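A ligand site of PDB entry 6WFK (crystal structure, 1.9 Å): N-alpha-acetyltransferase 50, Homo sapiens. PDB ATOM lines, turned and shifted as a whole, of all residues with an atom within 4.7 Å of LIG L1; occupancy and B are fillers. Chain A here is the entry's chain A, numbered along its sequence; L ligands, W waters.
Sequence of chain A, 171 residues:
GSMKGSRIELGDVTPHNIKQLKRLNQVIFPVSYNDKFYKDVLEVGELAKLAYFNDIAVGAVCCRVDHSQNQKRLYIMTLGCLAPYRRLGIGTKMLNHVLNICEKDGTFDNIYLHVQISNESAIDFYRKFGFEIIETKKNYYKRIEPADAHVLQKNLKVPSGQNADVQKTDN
Phe 29 touches LIG L1. Pro 30 touches LIG L1. Val 31 touches LIG L1 (CG2 to O1, 3.4 Å). Phe 37 touches LIG L1. NE of Arg 64 touches C23 of LIG L1, at 3.5 Å. Tyr 75 touches LIG L1. Val 115 touches LIG L1. Hydrophobic or aromatic side chains that line LIG L1: Phe 29, Pro 30, Val 31, Tyr 33, Phe 37, Tyr 75, Met 77, Tyr 140 and Tyr 141. The nearest printed residue that does not touch LIG L1 is Ile 144 (4.1 Å).
ND1 of His 114 lies within hydrogen-bond range of OH of Tyr 75 (2.8 Å). OH of Tyr 140 is in hydrogen-bond range of OH of Tyr 75 (3.3 Å). The backbone NH of Tyr 75 sits at hydrogen-bond distance from the backbone carbonyl oxygen of Arg 64 (2.9 Å).
Water W1 bridges a nitrogen (N3) of LIG L1 (2.8 Å) and the backbone NH (N) of Ser 32 (2.9 Å). Water W2 lies within hydrogen-bond range of ND2 of Asn 119 (2.8 Å), O2 of LIG L1 (2.9 Å) and OE1 of Gln 116 (3.4 Å). Water W4 lies within hydrogen-bond range of N of His 114, OH of Tyr 75 and N10 of LIG L1.
O of His 114 lies within hydrogen-bond range of N6 of LIG L1 (2.7 Å). An oxygen (O5) of LIG L1 is in hydrogen-bond range of the side-chain hydroxyl of Tyr 141 (2.7 Å). O of Met 77 sits at hydrogen-bond distance from N10 of LIG L1, at 2.7 Å. N of Arg 143 lies within hydrogen-bond range of N4 of LIG L1, 2.9 Å away. The backbone NH (N) of Lys 142 sits at hydrogen-bond distance from a nitrogen (N1) of LIG L1 (2.9 Å). The side-chain hydroxyl of Tyr 33 sits at hydrogen-bond distance from an oxygen (O1) of LIG L1. O2 of LIG L1 sits at hydrogen-bond distance from N of Gln 116. The side-chain hydroxyl of Tyr 140 sits close to an oxygen (O3) of LIG L1, 3.4 Å away. An oxygen (O16) of LG2 L2 lies within hydrogen-bond range of the side-chain amide nitrogen (ND2) of Asn 119 (2.5 Å).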
ATOM      1  N   PHE A  29       6.101 -11.263  27.490  1.00  0.00           N
ATOM      2  CA  PHE A  29       5.298 -10.065  27.720  1.00  0.00           C
ATOM      3  C   PHE A  29       4.002 -10.287  28.479  1.00  0.00           C
ATOM      4  O   PHE A  29       3.335 -11.312  28.294  1.00  0.00           O
ATOM      5  CB  PHE A  29       5.056  -9.322  26.399  1.00  0.00           C
ATOM      6  CG  PHE A  29       6.380  -8.892  25.776  1.00  0.00           C
ATOM      7  CD1 PHE A  29       7.195  -7.949  26.411  1.00  0.00           C
ATOM      8  CD2 PHE A  29       6.851  -9.505  24.615  1.00  0.00           C
ATOM      9  CE1 PHE A  29       8.429  -7.594  25.872  1.00  0.00           C
ATOM     10  CE2 PHE A  29       8.087  -9.139  24.067  1.00  0.00           C
ATOM     11  CZ  PHE A  29       8.856  -8.173  24.698  1.00  0.00           C
ATOM     12  N   PRO A  30       3.610  -9.295  29.341  1.00  0.00           N
ATOM     13  CA  PRO A  30       2.376  -9.459  30.132  1.00  0.00           C
ATOM     14  C   PRO A  30       1.087  -9.192  29.361  1.00  0.00           C
ATOM     15  O   PRO A  30       0.009  -9.442  29.884  1.00  0.00           O
ATOM     16  CB  PRO A  30       2.585  -8.461  31.296  1.00  0.00           C
ATOM     17  CG  PRO A  30       3.429  -7.408  30.727  1.00  0.00           C
ATOM     18  CD  PRO A  30       4.308  -8.048  29.688  1.00  0.00           C
ATOM     19  N   VAL A  31       1.199  -8.624  28.156  1.00  0.00           N
ATOM     20  CA  VAL A  31       0.066  -8.311  27.279  1.00  0.00           C
ATOM     21  C   VAL A  31       0.122  -9.207  26.027  1.00  0.00           C
ATOM     22  O   VAL A  31       1.207  -9.673  25.657  1.00  0.00           O
ATOM     23  CB  VAL A  31      -0.020  -6.778  26.916  1.00  0.00           C
ATOM     24  CG1 VAL A  31      -0.130  -5.915  28.175  1.00  0.00           C
ATOM     25  CG2 VAL A  31       1.159  -6.334  26.069  1.00  0.00           C
ATOM     26  N   SER A  32      -1.041  -9.431  25.393  1.00  0.00           N
ATOM     27  CA  SER A  32      -1.191 -10.239  24.177  1.00  0.00           C
ATOM     28  C   SER A  32      -1.108  -9.360  22.935  1.00  0.00           C
ATOM     29  O   SER A  32      -1.513  -8.200  22.969  1.00  0.00           O
ATOM     30  CB  SER A  32      -2.529 -10.976  24.183  1.00  0.00           C
ATOM     31  OG  SER A  32      -2.510 -12.013  25.150  1.00  0.00           O
ATOM     32  N   TYR A  33      -0.581  -9.921  21.843  1.00  0.00           N
ATOM     33  CA  TYR A  33      -0.491  -9.190  20.573  1.00  0.00           C
ATOM     34  C   TYR A  33      -1.379  -9.921  19.574  1.00  0.00           C
ATOM     35  O   TYR A  33      -1.367 -11.143  19.546  1.00  0.00           O
ATOM     36  CB  TYR A  33       0.972  -9.017  20.123  1.00  0.00           C
ATOM     37  CG  TYR A  33       1.710  -8.098  21.064  1.00  0.00           C
ATOM     38  CD1 TYR A  33       1.698  -6.721  20.859  1.00  0.00           C
ATOM     39  CD2 TYR A  33       2.318  -8.583  22.221  1.00  0.00           C
ATOM     40  CE1 TYR A  33       2.316  -5.852  21.766  1.00  0.00           C
ATOM     41  CE2 TYR A  33       2.911  -7.719  23.141  1.00  0.00           C
ATOM     42  CZ  TYR A  33       2.890  -6.351  22.914  1.00  0.00           C
ATOM     43  OH  TYR A  33       3.500  -5.503  23.796  1.00  0.00           O
ATOM     44  N   PHE A  37      -0.797  -7.713  14.422  1.00  0.00           N
ATOM     45  CA  PHE A  37       0.563  -7.409  14.855  1.00  0.00           C
ATOM     46  C   PHE A  37       1.535  -8.368  14.147  1.00  0.00           C
ATOM     47  O   PHE A  37       2.507  -7.914  13.548  1.00  0.00           O
ATOM     48  CB  PHE A  37       0.694  -7.522  16.384  1.00  0.00           C
ATOM     49  CG  PHE A  37       2.097  -7.416  16.942  1.00  0.00           C
ATOM     50  CD1 PHE A  37       2.632  -6.170  17.284  1.00  0.00           C
ATOM     51  CD2 PHE A  37       2.883  -8.549  17.111  1.00  0.00           C
ATOM     52  CE1 PHE A  37       3.931  -6.078  17.787  1.00  0.00           C
ATOM     53  CE2 PHE A  37       4.188  -8.435  17.619  1.00  0.00           C
ATOM     54  CZ  PHE A  37       4.700  -7.210  17.954  1.00  0.00           C
ATOM     55  N   ASP A  40       1.667  -7.785  10.346  1.00  0.00           N
ATOM     56  CA  ASP A  40       2.464  -6.572  10.117  1.00  0.00           C
ATOM     57  C   ASP A  40       3.965  -6.879  10.248  1.00  0.00           C
ATOM     58  O   ASP A  40       4.739  -6.395   9.435  1.00  0.00           O
ATOM     59  CB  ASP A  40       2.080  -5.470  11.119  1.00  0.00           C
ATOM     60  CG  ASP A  40       0.706  -4.848  10.927  1.00  0.00           C
ATOM     61  OD1 ASP A  40       0.147  -4.957   9.808  1.00  0.00           O
ATOM     62  OD2 ASP A  40       0.178  -4.248  11.901  1.00  0.00           O
ATOM     63  N   ARG A  64       8.098  -0.735  14.069  1.00  0.00           N
ATOM     64  CA  ARG A  64       7.317  -0.172  12.962  1.00  0.00           C
ATOM     65  C   ARG A  64       7.779   1.253  12.749  1.00  0.00           C
ATOM     66  O   ARG A  64       8.326   1.886  13.666  1.00  0.00           O
ATOM     67  CB  ARG A  64       5.789  -0.237  13.223  1.00  0.00           C
ATOM     68  CG  ARG A  64       5.259   0.695  14.320  1.00  0.00           C
ATOM     69  CD  ARG A  64       3.747   0.662  14.511  1.00  0.00           C
ATOM     70  NE  ARG A  64       3.028   1.025  13.292  1.00  0.00           N
ATOM     71  CZ  ARG A  64       2.786   2.284  12.913  1.00  0.00           C
ATOM     72  NH1 ARG A  64       3.172   3.305  13.666  1.00  0.00           N
ATOM     73  NH2 ARG A  64       2.153   2.521  11.759  1.00  0.00           N
ATOM     74  N   TYR A  75       9.324   3.177  16.013  1.00  0.00           N
ATOM     75  CA  TYR A  75       8.636   2.726  17.193  1.00  0.00           C
ATOM     76  C   TYR A  75       8.932   1.254  17.520  1.00  0.00           C
ATOM     77  O   TYR A  75       8.542   0.351  16.772  1.00  0.00           O
ATOM     78  CB  TYR A  75       7.114   3.026  17.083  1.00  0.00           C
ATOM     79  CG  TYR A  75       6.345   2.658  18.324  1.00  0.00           C
ATOM     80  CD1 TYR A  75       6.688   3.190  19.569  1.00  0.00           C
ATOM     81  CD2 TYR A  75       5.264   1.778  18.261  1.00  0.00           C
ATOM     82  CE1 TYR A  75       5.946   2.880  20.707  1.00  0.00           C
ATOM     83  CE2 TYR A  75       4.566   1.421  19.406  1.00  0.00           C
ATOM     84  CZ  TYR A  75       4.896   1.986  20.622  1.00  0.00           C
ATOM     85  OH  TYR A  75       4.228   1.617  21.759  1.00  0.00           O
ATOM     86  N   MET A  77       8.020  -1.814  19.292  1.00  0.00           N
ATOM     87  CA  MET A  77       6.800  -2.338  19.910  1.00  0.00           C
ATOM     88  C   MET A  77       7.132  -3.356  20.972  1.00  0.00           C
ATOM     89  O   MET A  77       6.568  -3.313  22.069  1.00  0.00           O
ATOM     90  CB  MET A  77       5.852  -2.925  18.860  1.00  0.00           C
ATOM     91  CG  MET A  77       5.315  -1.877  17.897  1.00  0.00           C
ATOM     92  SD  MET A  77       4.287  -2.581  16.592  1.00  0.00           S
ATOM     93  CE  MET A  77       5.527  -3.321  15.583  1.00  0.00           C
ATOM     94  N   THR A  78       8.035  -4.285  20.656  1.00  0.00           N
ATOM     95  CA  THR A  78       8.473  -5.323  21.583  1.00  0.00           C
ATOM     96  C   THR A  78       9.955  -5.586  21.382  1.00  0.00           C
ATOM     97  O   THR A  78      10.444  -5.624  20.245  1.00  0.00           O
ATOM     98  CB  THR A  78       7.695  -6.645  21.386  1.00  0.00           C
ATOM     99  OG1 THR A  78       7.796  -7.027  20.029  1.00  0.00           O
ATOM    100  CG2 THR A  78       6.237  -6.583  21.804  1.00  0.00           C
ATOM    101  N   HIS A 114       7.263   2.299  24.649  1.00  0.00           N
ATOM    102  CA  HIS A 114       6.578   2.378  25.919  1.00  0.00           C
ATOM    103  C   HIS A 114       7.160   1.341  26.849  1.00  0.00           C
ATOM    104  O   HIS A 114       7.462   0.222  26.422  1.00  0.00           O
ATOM    105  CB  HIS A 114       5.054   2.218  25.778  1.00  0.00           C
ATOM    106  CG  HIS A 114       4.408   3.409  25.136  1.00  0.00           C
ATOM    107  ND1 HIS A 114       4.373   3.553  23.765  1.00  0.00           N
ATOM    108  CD2 HIS A 114       3.848   4.504  25.709  1.00  0.00           C
ATOM    109  CE1 HIS A 114       3.759   4.710  23.533  1.00  0.00           C
ATOM    110  NE2 HIS A 114       3.418   5.309  24.678  1.00  0.00           N
ATOM    111  N   VAL A 115       7.385   1.714  28.119  1.00  0.00           N
ATOM    112  CA  VAL A 115       7.916   0.789  29.114  1.00  0.00           C
ATOM    113  C   VAL A 115       7.027   0.921  30.348  1.00  0.00           C
ATOM    114  O   VAL A 115       6.960   2.013  30.934  1.00  0.00           O
ATOM    115  CB  VAL A 115       9.421   1.052  29.501  1.00  0.00           C
ATOM    116  CG1 VAL A 115       9.893   0.034  30.522  1.00  0.00           C
ATOM    117  CG2 VAL A 115      10.336   1.052  28.273  1.00  0.00           C
ATOM    118  N   GLN A 116       6.346  -0.164  30.733  1.00  0.00           N
ATOM    119  CA  GLN A 116       5.513  -0.231  31.941  1.00  0.00           C
ATOM    120  C   GLN A 116       6.373   0.298  33.115  1.00  0.00           C
ATOM    121  O   GLN A 116       7.509  -0.117  33.257  1.00  0.00           O
ATOM    122  CB  GLN A 116       5.076  -1.673  32.183  1.00  0.00           C
ATOM    123  CG  GLN A 116       3.920  -1.801  33.180  1.00  0.00           C
ATOM    124  CD  GLN A 116       3.556  -3.248  33.439  1.00  0.00           C
ATOM    125  OE1 GLN A 116       4.306  -4.197  33.130  1.00  0.00           O
ATOM    126  NE2 GLN A 116       2.388  -3.447  34.027  1.00  0.00           N
ATOM    127  N   ASN A 119       8.851  -1.790  35.270  1.00  0.00           N
ATOM    128  CA  ASN A 119       9.971  -2.440  34.606  1.00  0.00           C
ATOM    129  C   ASN A 119      11.260  -1.651  34.751  1.00  0.00           C
ATOM    130  O   ASN A 119      11.794  -1.097  33.784  1.00  0.00           O
ATOM    131  CB  ASN A 119       9.634  -2.720  33.144  1.00  0.00           C
ATOM    132  CG  ASN A 119      10.430  -3.879  32.621  1.00  0.00           C
ATOM    133  OD1 ASN A 119      11.517  -4.222  33.098  1.00  0.00           O
ATOM    134  ND2 ASN A 119       9.884  -4.496  31.614  1.00  0.00           N
ATOM    135  N   TYR A 140      -1.986   3.668  30.139  1.00  0.00           N
ATOM    136  CA  TYR A 140      -1.576   3.214  28.814  1.00  0.00           C
ATOM    137  C   TYR A 140      -2.088   1.772  28.610  1.00  0.00           C
ATOM    138  O   TYR A 140      -2.601   1.454  27.540  1.00  0.00           O
ATOM    139  CB  TYR A 140      -0.045   3.300  28.666  1.00  0.00           C
ATOM    140  CG  TYR A 140       0.421   2.775  27.334  1.00  0.00           C
ATOM    141  CD1 TYR A 140       0.275   3.537  26.180  1.00  0.00           C
ATOM    142  CD2 TYR A 140       0.934   1.483  27.208  1.00  0.00           C
ATOM    143  CE1 TYR A 140       0.627   3.021  24.926  1.00  0.00           C
ATOM    144  CE2 TYR A 140       1.290   0.964  25.963  1.00  0.00           C
ATOM    145  CZ  TYR A 140       1.159   1.742  24.830  1.00  0.00           C
ATOM    146  OH  TYR A 140       1.508   1.269  23.603  1.00  0.00           O
ATOM    147  N   TYR A 141      -1.963   0.925  29.640  1.00  0.00           N
ATOM    148  CA  TYR A 141      -2.425  -0.458  29.641  1.00  0.00           C
ATOM    149  C   TYR A 141      -3.822  -0.515  30.236  1.00  0.00           C
ATOM    150  O   TYR A 141      -4.166   0.299  31.097  1.00  0.00           O
ATOM    151  CB  TYR A 141      -1.462  -1.374  30.413  1.00  0.00           C
ATOM    152  CG  TYR A 141      -0.045  -1.313  29.892  1.00  0.00           C
ATOM    153  CD1 TYR A 141       0.309  -1.914  28.691  1.00  0.00           C
ATOM    154  CD2 TYR A 141       0.949  -0.642  30.611  1.00  0.00           C
ATOM    155  CE1 TYR A 141       1.611  -1.836  28.203  1.00  0.00           C
ATOM    156  CE2 TYR A 141       2.256  -0.566  30.131  1.00  0.00           C
ATOM    157  CZ  TYR A 141       2.572  -1.140  28.913  1.00  0.00           C
ATOM    158  OH  TYR A 141       3.847  -1.016  28.418  1.00  0.00           O
ATOM    159  N   LYS A 142      -4.637  -1.478  29.773  1.00  0.00           N
ATOM    160  CA  LYS A 142      -6.023  -1.584  30.228  1.00  0.00           C
ATOM    161  C   LYS A 142      -6.275  -2.716  31.194  1.00  0.00           C
ATOM    162  O   LYS A 142      -6.928  -2.497  32.207  1.00  0.00           O
ATOM    163  CB  LYS A 142      -6.987  -1.653  29.013  1.00  0.00           C
ATOM    164  CG  LYS A 142      -6.690  -0.635  27.902  1.00  0.00           C
ATOM    165  CD  LYS A 142      -6.875   0.828  28.354  1.00  0.00           C
ATOM    166  CE  LYS A 142      -6.170   1.803  27.456  1.00  0.00           C
ATOM    167  NZ  LYS A 142      -6.347   3.200  27.930  1.00  0.00           N
ATOM    168  N   ARG A 143      -5.699  -3.906  30.925  1.00  0.00           N
ATOM    169  CA  ARG A 143      -5.944  -5.097  31.737  1.00  0.00           C
ATOM    170  C   ARG A 143      -4.791  -5.496  32.670  1.00  0.00           C
ATOM    171  O   ARG A 143      -4.913  -6.501  33.380  1.00  0.00           O
ATOM    172  CB  ARG A 143      -6.338  -6.282  30.827  1.00  0.00           C
ATOM    173  CG  ARG A 143      -7.596  -6.031  29.998  1.00  0.00           C
ATOM    174  CD  ARG A 143      -8.585  -7.186  30.067  1.00  0.00           C
ATOM    175  NE  ARG A 143      -9.897  -6.813  29.534  1.00  0.00           N
ATOM    176  N   ILE A 144      -3.691  -4.737  32.695  1.00  0.00           N
ATOM    177  CA  ILE A 144      -2.572  -5.101  33.587  1.00  0.00           C
ATOM    178  C   ILE A 144      -2.213  -3.950  34.528  1.00  0.00           C
ATOM    179  O   ILE A 144      -2.497  -2.791  34.222  1.00  0.00           O
ATOM    180  CB  ILE A 144      -1.318  -5.699  32.843  1.00  0.00           C
ATOM    181  CG1 ILE A 144      -0.672  -4.671  31.875  1.00  0.00           C
ATOM    182  CG2 ILE A 144      -1.628  -7.016  32.152  1.00  0.00           C
ATOM    183  CD1 ILE A 144       0.821  -4.900  31.596  1.00  0.00           C
HETATM  184  C1  LIG L   1      -1.631  -4.006  24.735  1.00  0.00           C
HETATM  185  C2  LIG L   1      -2.164  -1.866  25.661  1.00  0.00           C
HETATM  186  C3  LIG L   1      -0.926  -3.401  23.715  1.00  0.00           C
HETATM  187  C4  LIG L   1      -1.461  -1.258  24.655  1.00  0.00           C
HETATM  188  C5  LIG L   1       0.696  -2.822  18.049  1.00  0.00           C
HETATM  189  C6  LIG L   1      -2.258  -3.240  25.700  1.00  0.00           C
HETATM  190  C7  LIG L   1      -0.846  -2.026  23.696  1.00  0.00           C
HETATM  191  C8  LIG L   1       0.920  -1.475  17.857  1.00  0.00           C
HETATM  192  C9  LIG L   1      -2.993  -3.917  26.796  1.00  0.00           C
HETATM  193  C10 LIG L   1       1.503  -1.591  19.969  1.00  0.00           C
HETATM  194  C11 LIG L   1       5.222  -4.767  26.630  1.00  0.00           C
HETATM  195  C12 LIG L   1       6.198  -2.920  27.889  1.00  0.00           C
HETATM  196  C13 LIG L   1      -0.114  -1.383  22.613  1.00  0.00           C
HETATM  197  C14 LIG L   1       0.687  -0.797  16.593  1.00  0.00           C
HETATM  198  C15 LIG L   1       4.844  -2.180  24.993  1.00  0.00           C
HETATM  199  C16 LIG L   1       6.048  -4.296  25.464  1.00  0.00           C
HETATM  200  C17 LIG L   1       3.399  -1.599  21.573  1.00  0.00           C
HETATM  201  C18 LIG L   1       2.130  -2.187  23.455  1.00  0.00           C
HETATM  202  C19 LIG L   1       1.971  -1.185  21.306  1.00  0.00           C
HETATM  203  C20 LIG L   1       6.161  -2.786  25.400  1.00  0.00           C
HETATM  204  C21 LIG L   1       3.449  -1.550  23.081  1.00  0.00           C
HETATM  205  C22 LIG L   1       4.514  -4.326  28.923  1.00  0.00           C
HETATM  206  C23 LIG L   1       0.411   1.458  15.610  1.00  0.00           C
HETATM  207  N1  LIG L   1      -3.395  -3.299  27.922  1.00  0.00           N
HETATM  208  N2  LIG L   1       1.375  -0.778  18.953  1.00  0.00           N
HETATM  209  N3  LIG L   1      -3.274  -5.239  26.801  1.00  0.00           N
HETATM  210  N4  LIG L   1      -3.947  -4.281  28.674  1.00  0.00           N
HETATM  211  N5  LIG L   1      -3.876  -5.462  27.997  1.00  0.00           N
HETATM  212  N6  LIG L   1       6.531  -2.294  26.700  1.00  0.00           N
HETATM  213  N7  LIG L   1       5.313  -3.985  27.764  1.00  0.00           N
HETATM  214  N8  LIG L   1       1.224  -1.736  22.427  1.00  0.00           N
HETATM  215  N9  LIG L   1       0.616   0.572  16.738  1.00  0.00           N
HETATM  216  N10 LIG L   1       4.598  -2.226  23.640  1.00  0.00           N
HETATM  217  O1  LIG L   1       4.521  -5.770  26.531  1.00  0.00           O
HETATM  218  O2  LIG L   1       6.651  -2.579  28.975  1.00  0.00           O
HETATM  219  O3  LIG L   1      -0.728  -0.591  21.917  1.00  0.00           O
HETATM  220  O4  LIG L   1       0.572  -1.412  15.539  1.00  0.00           O
HETATM  221  O5  LIG L   1       4.041  -1.701  25.782  1.00  0.00           O
HETATM  222  S1  LIG L   1       1.067  -3.227  19.682  1.00  0.00           S
HETATM  223  N1  LG2 L   2      19.566  -4.361  36.156  1.00  0.00           N
HETATM  224  C1  LG2 L   2      20.401  -3.364  35.858  1.00  0.00           C
HETATM  225  N2  LG2 L   2      20.874  -3.001  34.661  1.00  0.00           N
HETATM  226  C2  LG2 L   2      20.405  -3.801  33.693  1.00  0.00           C
HETATM  227  C3  LG2 L   2      19.559  -4.880  33.875  1.00  0.00           C
HETATM  228  C4  LG2 L   2      19.135  -5.155  35.170  1.00  0.00           C
HETATM  229  N3  LG2 L   2      18.289  -6.236  35.446  1.00  0.00           N
HETATM  230  N4  LG2 L   2      19.295  -5.494  32.678  1.00  0.00           N
HETATM  231  C5  LG2 L   2      19.973  -4.801  31.797  1.00  0.00           C
HETATM  232  N5  LG2 L   2      20.655  -3.751  32.349  1.00  0.00           N
HETATM  233  C6  LG2 L   2      21.620  -2.895  31.660  1.00  0.00           C
HETATM  234  C7  LG2 L   2      23.041  -3.268  32.026  1.00  0.00           C
HETATM  235  O1  LG2 L   2      23.927  -2.161  32.070  1.00  0.00           O
HETATM  236  C8  LG2 L   2      23.400  -4.258  30.934  1.00  0.00           C
HETATM  237  O2  LG2 L   2      24.802  -4.357  30.712  1.00  0.00           O
HETATM  238  P1  LG2 L   2      25.620  -5.483  31.566  1.00  0.00           P
HETATM  239  O3  LG2 L   2      26.948  -5.524  30.858  1.00  0.00           O
HETATM  240  O4  LG2 L   2      25.680  -4.892  32.974  1.00  0.00           O
HETATM  241  O5  LG2 L   2      24.788  -6.753  31.475  1.00  0.00           O
HETATM  242  C9  LG2 L   2      22.731  -3.653  29.731  1.00  0.00           C
HETATM  243  O6  LG2 L   2      21.531  -3.071  30.238  1.00  0.00           O
HETATM  244  C10 LG2 L   2      22.508  -4.637  28.591  1.00  0.00           C
HETATM  245  O7  LG2 L   2      21.942  -5.885  29.003  1.00  0.00           O
HETATM  246  P2  LG2 L   2      21.804  -7.096  27.920  1.00  0.00           P
HETATM  247  O8  LG2 L   2      22.366  -8.371  28.474  1.00  0.00           O
HETATM  248  O9  LG2 L   2      22.094  -6.662  26.525  1.00  0.00           O
HETATM  249  O10 LG2 L   2      20.166  -7.132  28.001  1.00  0.00           O
HETATM  250  P3  LG2 L   2      19.090  -8.343  28.100  1.00  0.00           P
HETATM  251  O11 LG2 L   2      19.370  -9.346  27.022  1.00  0.00           O
HETATM  252  O12 LG2 L   2      19.090  -8.809  29.538  1.00  0.00           O
HETATM  253  O13 LG2 L   2      17.795  -7.468  27.627  1.00  0.00           O
HETATM  254  C11 LG2 L   2      15.685  -6.561  28.338  1.00  0.00           C
HETATM  255  C12 LG2 L   2      17.202  -6.417  28.394  1.00  0.00           C
HETATM  256  C13 LG2 L   2      15.077  -5.324  28.949  1.00  0.00           C
HETATM  257  C14 LG2 L   2      15.251  -6.587  26.870  1.00  0.00           C
HETATM  258  C15 LG2 L   2      15.281  -7.837  29.102  1.00  0.00           C
HETATM  259  O14 LG2 L   2      15.407  -7.691  30.507  1.00  0.00           O
HETATM  260  C16 LG2 L   2      13.915  -8.413  28.833  1.00  0.00           C
HETATM  261  O15 LG2 L   2      13.772  -9.278  27.985  1.00  0.00           O
HETATM  262  N6  LG2 L   2      12.869  -7.963  29.604  1.00  0.00           N
HETATM  263  C17 LG2 L   2      11.493  -8.152  29.182  1.00  0.00           C
HETATM  264  C18 LG2 L   2      11.177  -7.329  27.952  1.00  0.00           C
HETATM  265  C19 LG2 L   2      10.832  -5.947  28.371  1.00  0.00           C
HETATM  266  O16 LG2 L   2      10.407  -5.782  29.490  1.00  0.00           O
HETATM  267  N7  LG2 L   2      10.977  -4.933  27.437  1.00  0.00           N
HETATM  268  C20 LG2 L   2       9.981  -3.874  27.430  1.00  0.00           C
HETATM  269  C21 LG2 L   2      10.232  -2.799  26.410  1.00  0.00           C
HETATM  270  S1  LG2 L   2       9.720  -3.440  24.795  1.00  0.00           S
HETATM  271  O   HOH W   1      -3.367  -7.762  25.559  1.00  0.00           O
HETATM  272  O   HOH W   2       7.136  -4.212  31.307  1.00  0.00           O
HETATM  273  O   HOH W   3      -3.957  -8.910  28.404  1.00  0.00           O
HETATM  274  O   HOH W   4       6.496   0.263  22.881  1.00  0.00           O
